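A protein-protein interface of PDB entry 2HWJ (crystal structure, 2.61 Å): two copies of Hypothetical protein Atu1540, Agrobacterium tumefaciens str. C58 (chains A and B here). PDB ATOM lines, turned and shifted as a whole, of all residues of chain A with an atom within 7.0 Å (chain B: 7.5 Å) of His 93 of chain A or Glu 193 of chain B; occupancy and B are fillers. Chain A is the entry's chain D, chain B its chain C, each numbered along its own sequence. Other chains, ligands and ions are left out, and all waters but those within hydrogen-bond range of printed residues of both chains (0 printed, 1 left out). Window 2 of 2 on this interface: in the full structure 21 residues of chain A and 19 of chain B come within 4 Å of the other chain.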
ATOM      1  N   ALA A  57     -17.445 -26.232 -16.572  1.00  0.00           N
ATOM      2  CA  ALA A  57     -16.889 -24.872 -16.639  1.00  0.00           C
ATOM      3  C   ALA A  57     -15.787 -24.822 -15.613  1.00  0.00           C
ATOM      4  O   ALA A  57     -15.979 -25.147 -14.426  1.00  0.00           O
ATOM      5  CB  ALA A  57     -17.911 -23.861 -16.383  1.00  0.00           C
ATOM      6  N   GLY A  58     -14.596 -24.484 -16.076  1.00  0.00           N
ATOM      7  CA  GLY A  58     -13.453 -24.504 -15.167  1.00  0.00           C
ATOM      8  C   GLY A  58     -12.987 -23.154 -14.675  1.00  0.00           C
ATOM      9  O   GLY A  58     -13.641 -22.130 -14.898  1.00  0.00           O
ATOM     10  N   PRO A  59     -11.833 -23.140 -14.001  1.00  0.00           N
ATOM     11  CA  PRO A  59     -11.369 -21.850 -13.530  1.00  0.00           C
ATOM     12  C   PRO A  59     -10.908 -21.144 -14.750  1.00  0.00           C
ATOM     13  O   PRO A  59     -10.560 -21.803 -15.782  1.00  0.00           O
ATOM     14  CB  PRO A  59     -10.191 -22.186 -12.615  1.00  0.00           C
ATOM     15  CG  PRO A  59     -10.330 -23.667 -12.346  1.00  0.00           C
ATOM     16  CD  PRO A  59     -10.909 -24.210 -13.630  1.00  0.00           C
ATOM     17  N   LYS A  90     -20.242 -26.642 -12.814  1.00  0.00           N
ATOM     18  CA  LYS A  90     -19.636 -25.346 -12.671  1.00  0.00           C
ATOM     19  C   LYS A  90     -18.614 -25.356 -11.505  1.00  0.00           C
ATOM     20  O   LYS A  90     -18.983 -25.406 -10.313  1.00  0.00           O
ATOM     21  CB  LYS A  90     -20.705 -24.280 -12.443  1.00  0.00           C
ATOM     22  CG  LYS A  90     -20.277 -22.932 -13.034  1.00  0.00           C
ATOM     23  CD  LYS A  90     -21.509 -22.052 -13.354  1.00  0.00           C
ATOM     24  CE  LYS A  90     -21.099 -20.612 -13.715  1.00  0.00           C
ATOM     25  NZ  LYS A  90     -21.011 -20.413 -15.210  1.00  0.00           N
ATOM     26  N   PHE A  91     -17.327 -25.309 -11.864  1.00  0.00           N
ATOM     27  CA  PHE A  91     -16.301 -25.242 -10.868  1.00  0.00           C
ATOM     28  C   PHE A  91     -15.504 -24.001 -11.032  1.00  0.00           C
ATOM     29  O   PHE A  91     -14.342 -23.992 -10.685  1.00  0.00           O
ATOM     30  CB  PHE A  91     -15.356 -26.404 -10.984  1.00  0.00           C
ATOM     31  CG  PHE A  91     -16.008 -27.725 -10.785  1.00  0.00           C
ATOM     32  CD1 PHE A  91     -16.924 -27.916  -9.795  1.00  0.00           C
ATOM     33  CD2 PHE A  91     -15.731 -28.790 -11.639  1.00  0.00           C
ATOM     34  CE1 PHE A  91     -17.546 -29.172  -9.626  1.00  0.00           C
ATOM     35  CE2 PHE A  91     -16.359 -30.033 -11.461  1.00  0.00           C
ATOM     36  CZ  PHE A  91     -17.232 -30.228 -10.439  1.00  0.00           C
ATOM     37  N   SER A  92     -16.111 -22.929 -11.501  1.00  0.00           N
ATOM     38  CA  SER A  92     -15.342 -21.727 -11.718  1.00  0.00           C
ATOM     39  C   SER A  92     -15.051 -20.918 -10.494  1.00  0.00           C
ATOM     40  O   SER A  92     -14.447 -19.885 -10.623  1.00  0.00           O
ATOM     41  CB  SER A  92     -15.966 -20.834 -12.781  1.00  0.00           C
ATOM     42  OG  SER A  92     -17.210 -21.346 -13.221  1.00  0.00           O
ATOM     43  N   HIS A  93     -15.435 -21.351  -9.306  1.00  0.00           N
ATOM     44  CA  HIS A  93     -15.162 -20.525  -8.155  1.00  0.00           C
ATOM     45  C   HIS A  93     -13.913 -20.994  -7.432  1.00  0.00           C
ATOM     46  O   HIS A  93     -13.516 -20.422  -6.392  1.00  0.00           O
ATOM     47  CB  HIS A  93     -16.369 -20.510  -7.228  1.00  0.00           C
ATOM     48  CG  HIS A  93     -16.842 -21.874  -6.878  1.00  0.00           C
ATOM     49  ND1 HIS A  93     -17.594 -22.638  -7.745  1.00  0.00           N
ATOM     50  CD2 HIS A  93     -16.619 -22.641  -5.788  1.00  0.00           C
ATOM     51  CE1 HIS A  93     -17.843 -23.809  -7.182  1.00  0.00           C
ATOM     52  NE2 HIS A  93     -17.257 -23.836  -5.997  1.00  0.00           N
ATOM     53  N   LEU A  94     -13.332 -22.056  -7.983  1.00  0.00           N
ATOM     54  CA  LEU A  94     -12.117 -22.687  -7.467  1.00  0.00           C
ATOM     55  C   LEU A  94     -10.815 -22.138  -8.038  1.00  0.00           C
ATOM     56  O   LEU A  94     -10.741 -21.795  -9.222  1.00  0.00           O
ATOM     57  CB  LEU A  94     -12.119 -24.162  -7.834  1.00  0.00           C
ATOM     58  CG  LEU A  94     -13.298 -25.102  -7.514  1.00  0.00           C
ATOM     59  CD1 LEU A  94     -13.106 -26.494  -8.152  1.00  0.00           C
ATOM     60  CD2 LEU A  94     -13.526 -25.260  -6.035  1.00  0.00           C
ATOM     61  N   GLY A  95      -9.766 -22.125  -7.226  1.00  0.00           N
ATOM     62  CA  GLY A  95      -8.410 -21.958  -7.747  1.00  0.00           C
ATOM     63  C   GLY A  95      -8.011 -23.089  -8.658  1.00  0.00           C
ATOM     64  O   GLY A  95      -8.706 -24.074  -8.707  1.00  0.00           O
ATOM     65  N   GLU A  98      -6.937 -26.421  -6.914  1.00  0.00           N
ATOM     66  CA  GLU A  98      -8.066 -27.058  -6.297  1.00  0.00           C
ATOM     67  C   GLU A  98      -8.813 -27.709  -7.400  1.00  0.00           C
ATOM     68  O   GLU A  98      -9.211 -28.841  -7.296  1.00  0.00           O
ATOM     69  CB  GLU A  98      -8.967 -26.072  -5.576  1.00  0.00           C
ATOM     70  CG  GLU A  98      -9.875 -26.794  -4.674  1.00  0.00           C
ATOM     71  CD  GLU A  98     -10.578 -25.934  -3.684  1.00  0.00           C
ATOM     72  OE1 GLU A  98     -10.675 -24.703  -3.888  1.00  0.00           O
ATOM     73  OE2 GLU A  98     -11.052 -26.500  -2.665  1.00  0.00           O
ATOM     74  N   TRP B 161     -14.121 -33.198   1.166  1.00  0.00           N
ATOM     75  CA  TRP B 161     -14.336 -32.138   2.143  1.00  0.00           C
ATOM     76  C   TRP B 161     -13.040 -31.718   2.913  1.00  0.00           C
ATOM     77  O   TRP B 161     -12.851 -30.497   3.217  1.00  0.00           O
ATOM     78  CB  TRP B 161     -15.452 -32.509   3.173  1.00  0.00           C
ATOM     79  CG  TRP B 161     -16.891 -32.227   2.663  1.00  0.00           C
ATOM     80  CD1 TRP B 161     -17.714 -33.111   2.001  1.00  0.00           C
ATOM     81  CD2 TRP B 161     -17.604 -30.970   2.705  1.00  0.00           C
ATOM     82  NE1 TRP B 161     -18.863 -32.476   1.651  1.00  0.00           N
ATOM     83  CE2 TRP B 161     -18.836 -31.171   2.037  1.00  0.00           C
ATOM     84  CE3 TRP B 161     -17.320 -29.713   3.231  1.00  0.00           C
ATOM     85  CZ2 TRP B 161     -19.835 -30.162   1.915  1.00  0.00           C
ATOM     86  CZ3 TRP B 161     -18.324 -28.666   3.095  1.00  0.00           C
ATOM     87  CH2 TRP B 161     -19.572 -28.926   2.456  1.00  0.00           C
ATOM     88  N   PHE B 164     -11.199 -29.385   0.712  1.00  0.00           N
ATOM     89  CA  PHE B 164     -11.717 -28.075   0.716  1.00  0.00           C
ATOM     90  C   PHE B 164     -11.252 -27.269   1.975  1.00  0.00           C
ATOM     91  O   PHE B 164     -10.854 -26.079   1.952  1.00  0.00           O
ATOM     92  CB  PHE B 164     -13.177 -28.272   0.728  1.00  0.00           C
ATOM     93  CG  PHE B 164     -13.924 -27.054   0.699  1.00  0.00           C
ATOM     94  CD1 PHE B 164     -14.084 -26.345  -0.493  1.00  0.00           C
ATOM     95  CD2 PHE B 164     -14.524 -26.553   1.871  1.00  0.00           C
ATOM     96  CE1 PHE B 164     -14.914 -25.137  -0.512  1.00  0.00           C
ATOM     97  CE2 PHE B 164     -15.382 -25.368   1.843  1.00  0.00           C
ATOM     98  CZ  PHE B 164     -15.525 -24.694   0.679  1.00  0.00           C
ATOM     99  N   ARG B 168      -8.386 -23.758   3.173  1.00  0.00           N
ATOM    100  CA  ARG B 168      -9.062 -22.559   3.654  1.00  0.00           C
ATOM    101  C   ARG B 168      -8.952 -22.285   5.127  1.00  0.00           C
ATOM    102  O   ARG B 168      -9.287 -21.195   5.556  1.00  0.00           O
ATOM    103  CB  ARG B 168     -10.533 -22.600   3.269  1.00  0.00           C
ATOM    104  CG  ARG B 168     -10.716 -22.753   1.789  1.00  0.00           C
ATOM    105  CD  ARG B 168     -12.218 -22.901   1.481  1.00  0.00           C
ATOM    106  NE  ARG B 168     -12.422 -22.593   0.083  1.00  0.00           N
ATOM    107  CZ  ARG B 168     -12.051 -23.389  -0.928  1.00  0.00           C
ATOM    108  NH1 ARG B 168     -11.443 -24.607  -0.733  1.00  0.00           N
ATOM    109  NH2 ARG B 168     -12.287 -22.969  -2.154  1.00  0.00           N
ATOM    110  N   LYS B 187     -19.382 -22.500   8.771  1.00  0.00           N
ATOM    111  CA  LYS B 187     -19.833 -21.376   8.018  1.00  0.00           C
ATOM    112  C   LYS B 187     -19.427 -21.526   6.534  1.00  0.00           C
ATOM    113  O   LYS B 187     -20.242 -21.208   5.668  1.00  0.00           O
ATOM    114  CB  LYS B 187     -19.510 -20.044   8.746  1.00  0.00           C
ATOM    115  CG  LYS B 187     -18.361 -19.138   8.304  1.00  0.00           C
ATOM    116  CD  LYS B 187     -18.896 -18.172   7.220  1.00  0.00           C
ATOM    117  CE  LYS B 187     -17.953 -16.933   6.900  1.00  0.00           C
ATOM    118  NZ  LYS B 187     -17.795 -15.991   8.081  1.00  0.00           N
ATOM    119  N   LEU B 188     -18.291 -22.139   6.222  1.00  0.00           N
ATOM    120  CA  LEU B 188     -18.072 -22.565   4.824  1.00  0.00           C
ATOM    121  C   LEU B 188     -18.969 -23.701   4.320  1.00  0.00           C
ATOM    122  O   LEU B 188     -19.391 -23.688   3.172  1.00  0.00           O
ATOM    123  CB  LEU B 188     -16.635 -22.975   4.535  1.00  0.00           C
ATOM    124  CG  LEU B 188     -15.503 -22.013   4.943  1.00  0.00           C
ATOM    125  CD1 LEU B 188     -14.259 -22.778   5.242  1.00  0.00           C
ATOM    126  CD2 LEU B 188     -15.247 -20.931   3.928  1.00  0.00           C
ATOM    127  N   ALA B 189     -19.237 -24.715   5.136  1.00  0.00           N
ATOM    128  CA  ALA B 189     -20.084 -25.787   4.642  1.00  0.00           C
ATOM    129  C   ALA B 189     -21.385 -25.220   4.032  1.00  0.00           C
ATOM    130  O   ALA B 189     -21.770 -25.609   2.923  1.00  0.00           O
ATOM    131  CB  ALA B 189     -20.384 -26.707   5.684  1.00  0.00           C
ATOM    132  N   LYS B 190     -21.980 -24.263   4.742  1.00  0.00           N
ATOM    133  CA  LYS B 190     -23.235 -23.576   4.417  1.00  0.00           C
ATOM    134  C   LYS B 190     -23.197 -22.517   3.336  1.00  0.00           C
ATOM    135  O   LYS B 190     -24.203 -21.855   3.093  1.00  0.00           O
ATOM    136  CB  LYS B 190     -23.726 -22.835   5.663  1.00  0.00           C
ATOM    137  CG  LYS B 190     -24.145 -23.760   6.813  1.00  0.00           C
ATOM    138  CD  LYS B 190     -25.058 -24.841   6.200  1.00  0.00           C
ATOM    139  CE  LYS B 190     -25.330 -26.150   6.993  1.00  0.00           C
ATOM    140  NZ  LYS B 190     -25.026 -27.225   5.958  1.00  0.00           N
ATOM    141  N   SER B 191     -22.064 -22.261   2.726  1.00  0.00           N
ATOM    142  CA  SER B 191     -22.024 -21.128   1.836  1.00  0.00           C
ATOM    143  C   SER B 191     -21.832 -21.631   0.402  1.00  0.00           C
ATOM    144  O   SER B 191     -21.712 -22.856   0.192  1.00  0.00           O
ATOM    145  CB  SER B 191     -20.896 -20.224   2.261  1.00  0.00           C
ATOM    146  OG  SER B 191     -19.703 -20.866   1.986  1.00  0.00           O
ATOM    147  N   ARG B 192     -21.781 -20.719  -0.575  1.00  0.00           N
ATOM    148  CA  ARG B 192     -21.819 -21.121  -1.967  1.00  0.00           C
ATOM    149  C   ARG B 192     -20.419 -21.608  -2.304  1.00  0.00           C
ATOM    150  O   ARG B 192     -20.198 -22.390  -3.225  1.00  0.00           O
ATOM    151  CB  ARG B 192     -22.141 -19.944  -2.890  1.00  0.00           C
ATOM    152  CG  ARG B 192     -22.507 -18.555  -2.223  1.00  0.00           C
ATOM    153  CD  ARG B 192     -22.860 -17.340  -3.298  1.00  0.00           C
ATOM    154  NE  ARG B 192     -24.218 -17.545  -3.878  1.00  0.00           N
ATOM    155  CZ  ARG B 192     -25.369 -16.964  -3.460  1.00  0.00           C
ATOM    156  NH1 ARG B 192     -25.378 -16.064  -2.458  1.00  0.00           N
ATOM    157  NH2 ARG B 192     -26.532 -17.278  -4.066  1.00  0.00           N
ATOM    158  N   GLU B 193     -19.434 -21.179  -1.548  1.00  0.00           N
ATOM    159  CA  GLU B 193     -18.141 -21.711  -1.852  1.00  0.00           C
ATOM    160  C   GLU B 193     -18.086 -23.260  -1.906  1.00  0.00           C
ATOM    161  O   GLU B 193     -17.282 -23.806  -2.670  1.00  0.00           O
ATOM    162  CB  GLU B 193     -17.133 -21.140  -0.893  1.00  0.00           C
ATOM    163  CG  GLU B 193     -16.347 -20.048  -1.612  1.00  0.00           C
ATOM    164  CD  GLU B 193     -14.865 -20.424  -1.795  1.00  0.00           C
ATOM    165  OE1 GLU B 193     -14.119 -20.496  -0.747  1.00  0.00           O
ATOM    166  OE2 GLU B 193     -14.467 -20.629  -2.978  1.00  0.00           O
ATOM    167  N   ALA B 194     -18.950 -23.954  -1.136  1.00  0.00           N
ATOM    168  CA  ALA B 194     -18.818 -25.362  -0.966  1.00  0.00           C
ATOM    169  C   ALA B 194     -19.835 -26.153  -1.809  1.00  0.00           C
ATOM    170  O   ALA B 194     -19.892 -27.404  -1.745  1.00  0.00           O
ATOM    171  CB  ALA B 194     -18.962 -25.696   0.505  1.00  0.00           C
ATOM    172  N   ARG B 195     -20.613 -25.429  -2.602  1.00  0.00           N
ATOM    173  CA  ARG B 195     -21.690 -25.980  -3.386  1.00  0.00           C
ATOM    174  C   ARG B 195     -21.295 -27.115  -4.339  1.00  0.00           C
ATOM    175  O   ARG B 195     -22.101 -27.967  -4.682  1.00  0.00           O
ATOM    176  CB  ARG B 195     -22.410 -24.882  -4.196  1.00  0.00           C
ATOM    177  CG  ARG B 195     -23.838 -25.426  -4.582  1.00  0.00           C
ATOM    178  CD  ARG B 195     -24.611 -24.743  -5.799  1.00  0.00           C
ATOM    179  NE  ARG B 195     -25.461 -23.554  -5.499  1.00  0.00           N
ATOM    180  CZ  ARG B 195     -26.804 -23.526  -5.551  1.00  0.00           C
ATOM    181  NH1 ARG B 195     -27.499 -24.657  -5.826  1.00  0.00           N
ATOM    182  NH2 ARG B 195     -27.456 -22.356  -5.314  1.00  0.00           N
ATOM    183  N   HIS B 196     -20.077 -27.127  -4.802  1.00  0.00           N
ATOM    184  CA  HIS B 196     -19.693 -28.199  -5.681  1.00  0.00           C
ATOM    185  C   HIS B 196     -19.425 -29.473  -4.913  1.00  0.00           C
ATOM    186  O   HIS B 196     -19.067 -30.455  -5.512  1.00  0.00           O
ATOM    187  CB  HIS B 196     -18.378 -27.835  -6.383  1.00  0.00           C
ATOM    188  CG  HIS B 196     -17.292 -27.454  -5.424  1.00  0.00           C
ATOM    189  ND1 HIS B 196     -16.226 -28.287  -5.129  1.00  0.00           N
ATOM    190  CD2 HIS B 196     -17.163 -26.377  -4.616  1.00  0.00           C
ATOM    191  CE1 HIS B 196     -15.469 -27.735  -4.203  1.00  0.00           C
ATOM    192  NE2 HIS B 196     -16.020 -26.581  -3.871  1.00  0.00           N
ATOM    193  N   LEU B 197     -19.526 -29.512  -3.594  1.00  0.00           N
ATOM    194  CA  LEU B 197     -19.048 -30.715  -2.881  1.00  0.00           C
ATOM    195  C   LEU B 197     -20.147 -31.782  -2.658  1.00  0.00           C
ATOM    196  O   LEU B 197     -21.320 -31.500  -2.471  1.00  0.00           O
ATOM    197  CB  LEU B 197     -18.462 -30.260  -1.514  1.00  0.00           C
ATOM    198  CG  LEU B 197     -17.089 -29.590  -1.595  1.00  0.00           C
ATOM    199  CD1 LEU B 197     -16.622 -28.923  -0.305  1.00  0.00           C
ATOM    200  CD2 LEU B 197     -16.006 -30.638  -2.100  1.00  0.00           C
ATOM    201  N   TRP B 200     -23.468 -31.464  -0.162  1.00  0.00           N
ATOM    202  CA  TRP B 200     -23.654 -30.035   0.194  1.00  0.00           C
ATOM    203  C   TRP B 200     -25.045 -29.711   0.592  1.00  0.00           C
ATOM    204  O   TRP B 200     -25.978 -30.172   0.066  1.00  0.00           O
ATOM    205  CB  TRP B 200     -23.205 -29.086  -0.921  1.00  0.00           C
ATOM    206  CG  TRP B 200     -23.334 -27.632  -0.556  1.00  0.00           C
ATOM    207  CD1 TRP B 200     -22.460 -26.897   0.152  1.00  0.00           C
ATOM    208  CD2 TRP B 200     -24.404 -26.710  -0.898  1.00  0.00           C
ATOM    209  NE1 TRP B 200     -22.901 -25.565   0.323  1.00  0.00           N
ATOM    210  CE2 TRP B 200     -24.050 -25.424  -0.360  1.00  0.00           C
ATOM    211  CE3 TRP B 200     -25.633 -26.841  -1.614  1.00  0.00           C
ATOM    212  CZ2 TRP B 200     -24.858 -24.307  -0.479  1.00  0.00           C
ATOM    213  CZ3 TRP B 200     -26.471 -25.694  -1.747  1.00  0.00           C
ATOM    214  CH2 TRP B 200     -26.077 -24.426  -1.152  1.00  0.00           C
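Hydrophobic or aromatic side chains of chain A that line the printed part of chain B: Phe 91, His 93 and Leu 94.
Printed residues of chain B that touch a printed residue of chain A: Phe 164, Arg 168, Glu 193 and His 196.
Hydrophobic or aromatic side chains of chain B within 4 Å of the printed part of chain A: Phe 164 and His 196.
Among the printed residues, Asp or Glu carboxylates within 4 Å of a Lys or Arg side-chain nitrogen of the other chain: Glu 98 of chain A with Arg 168 of chain B.
No position is printed for both chains.
Of the 6 pairs that touch across the chains among the printed residues, none has its exchanged pair printed and touching as well.
Among the printed residues, pairs that only touch across the chains: His 93 of chain A with His 196 of chain B, Leu 94 of chain A with His 196 of chain B, Phe 91 of chain A with His 196 of chain B and Glu 98 of chain A with Phe 164 of chain B.
Of chain B, only Glu 193 (3.3 Å) and His 196 (2.9 Å) come within 4 Å of His 93 of chain A.
Glu 193 of chain B touches one residue of chain A.
Printed residues of chain B within 4 Å of Glu 98 of chain A: Phe 164 (3.7 Å) and Arg 168 (2.7 Å).
Of the printed residues of chain B, Phe 91 of chain A touches His 196 (3.6 Å).
Of the printed residues of chain B, Leu 94 of chain A touches His 196.
Of the printed residues of chain A, Arg 168 of chain B touches Glu 98 (2.7 Å).
Of the printed residues of chain A, His 196 of chain B touches Phe 91, His 93 and Leu 94.
The nearest residue of chain B that does not touch His 93 of chain A is Arg 192 of chain B (4.3 Å).
The nearest printed residue of chain B that does not touch Glu 98 of chain A is His 196 of chain B (4.8 Å).
O of Phe 164 of chain B sits at hydrogen-bond distance from NH1 of Arg 168 of chain B (3.1 Å).
The guanidinium group of Arg 168 of chain B lies within salt-bridge range of the side-chain carboxylate of Glu 193 of chain B.
O of Glu 193 of chain B sits close to NE2 of His 196 of chain B.
O of Ala 57 of chain A sits at hydrogen-bond distance from N of Phe 91 of chain A (2.9 Å).
The side-chain carboxylate (OE2) of Glu 98 of chain A lies within salt-bridge range of the guanidinium group (NH1) of Arg 168 of chain B (2.7 Å).
NE2 of His 93 of chain A lies within hydrogen-bond range of O of Glu 193 of chain B, at 3.3 Å.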
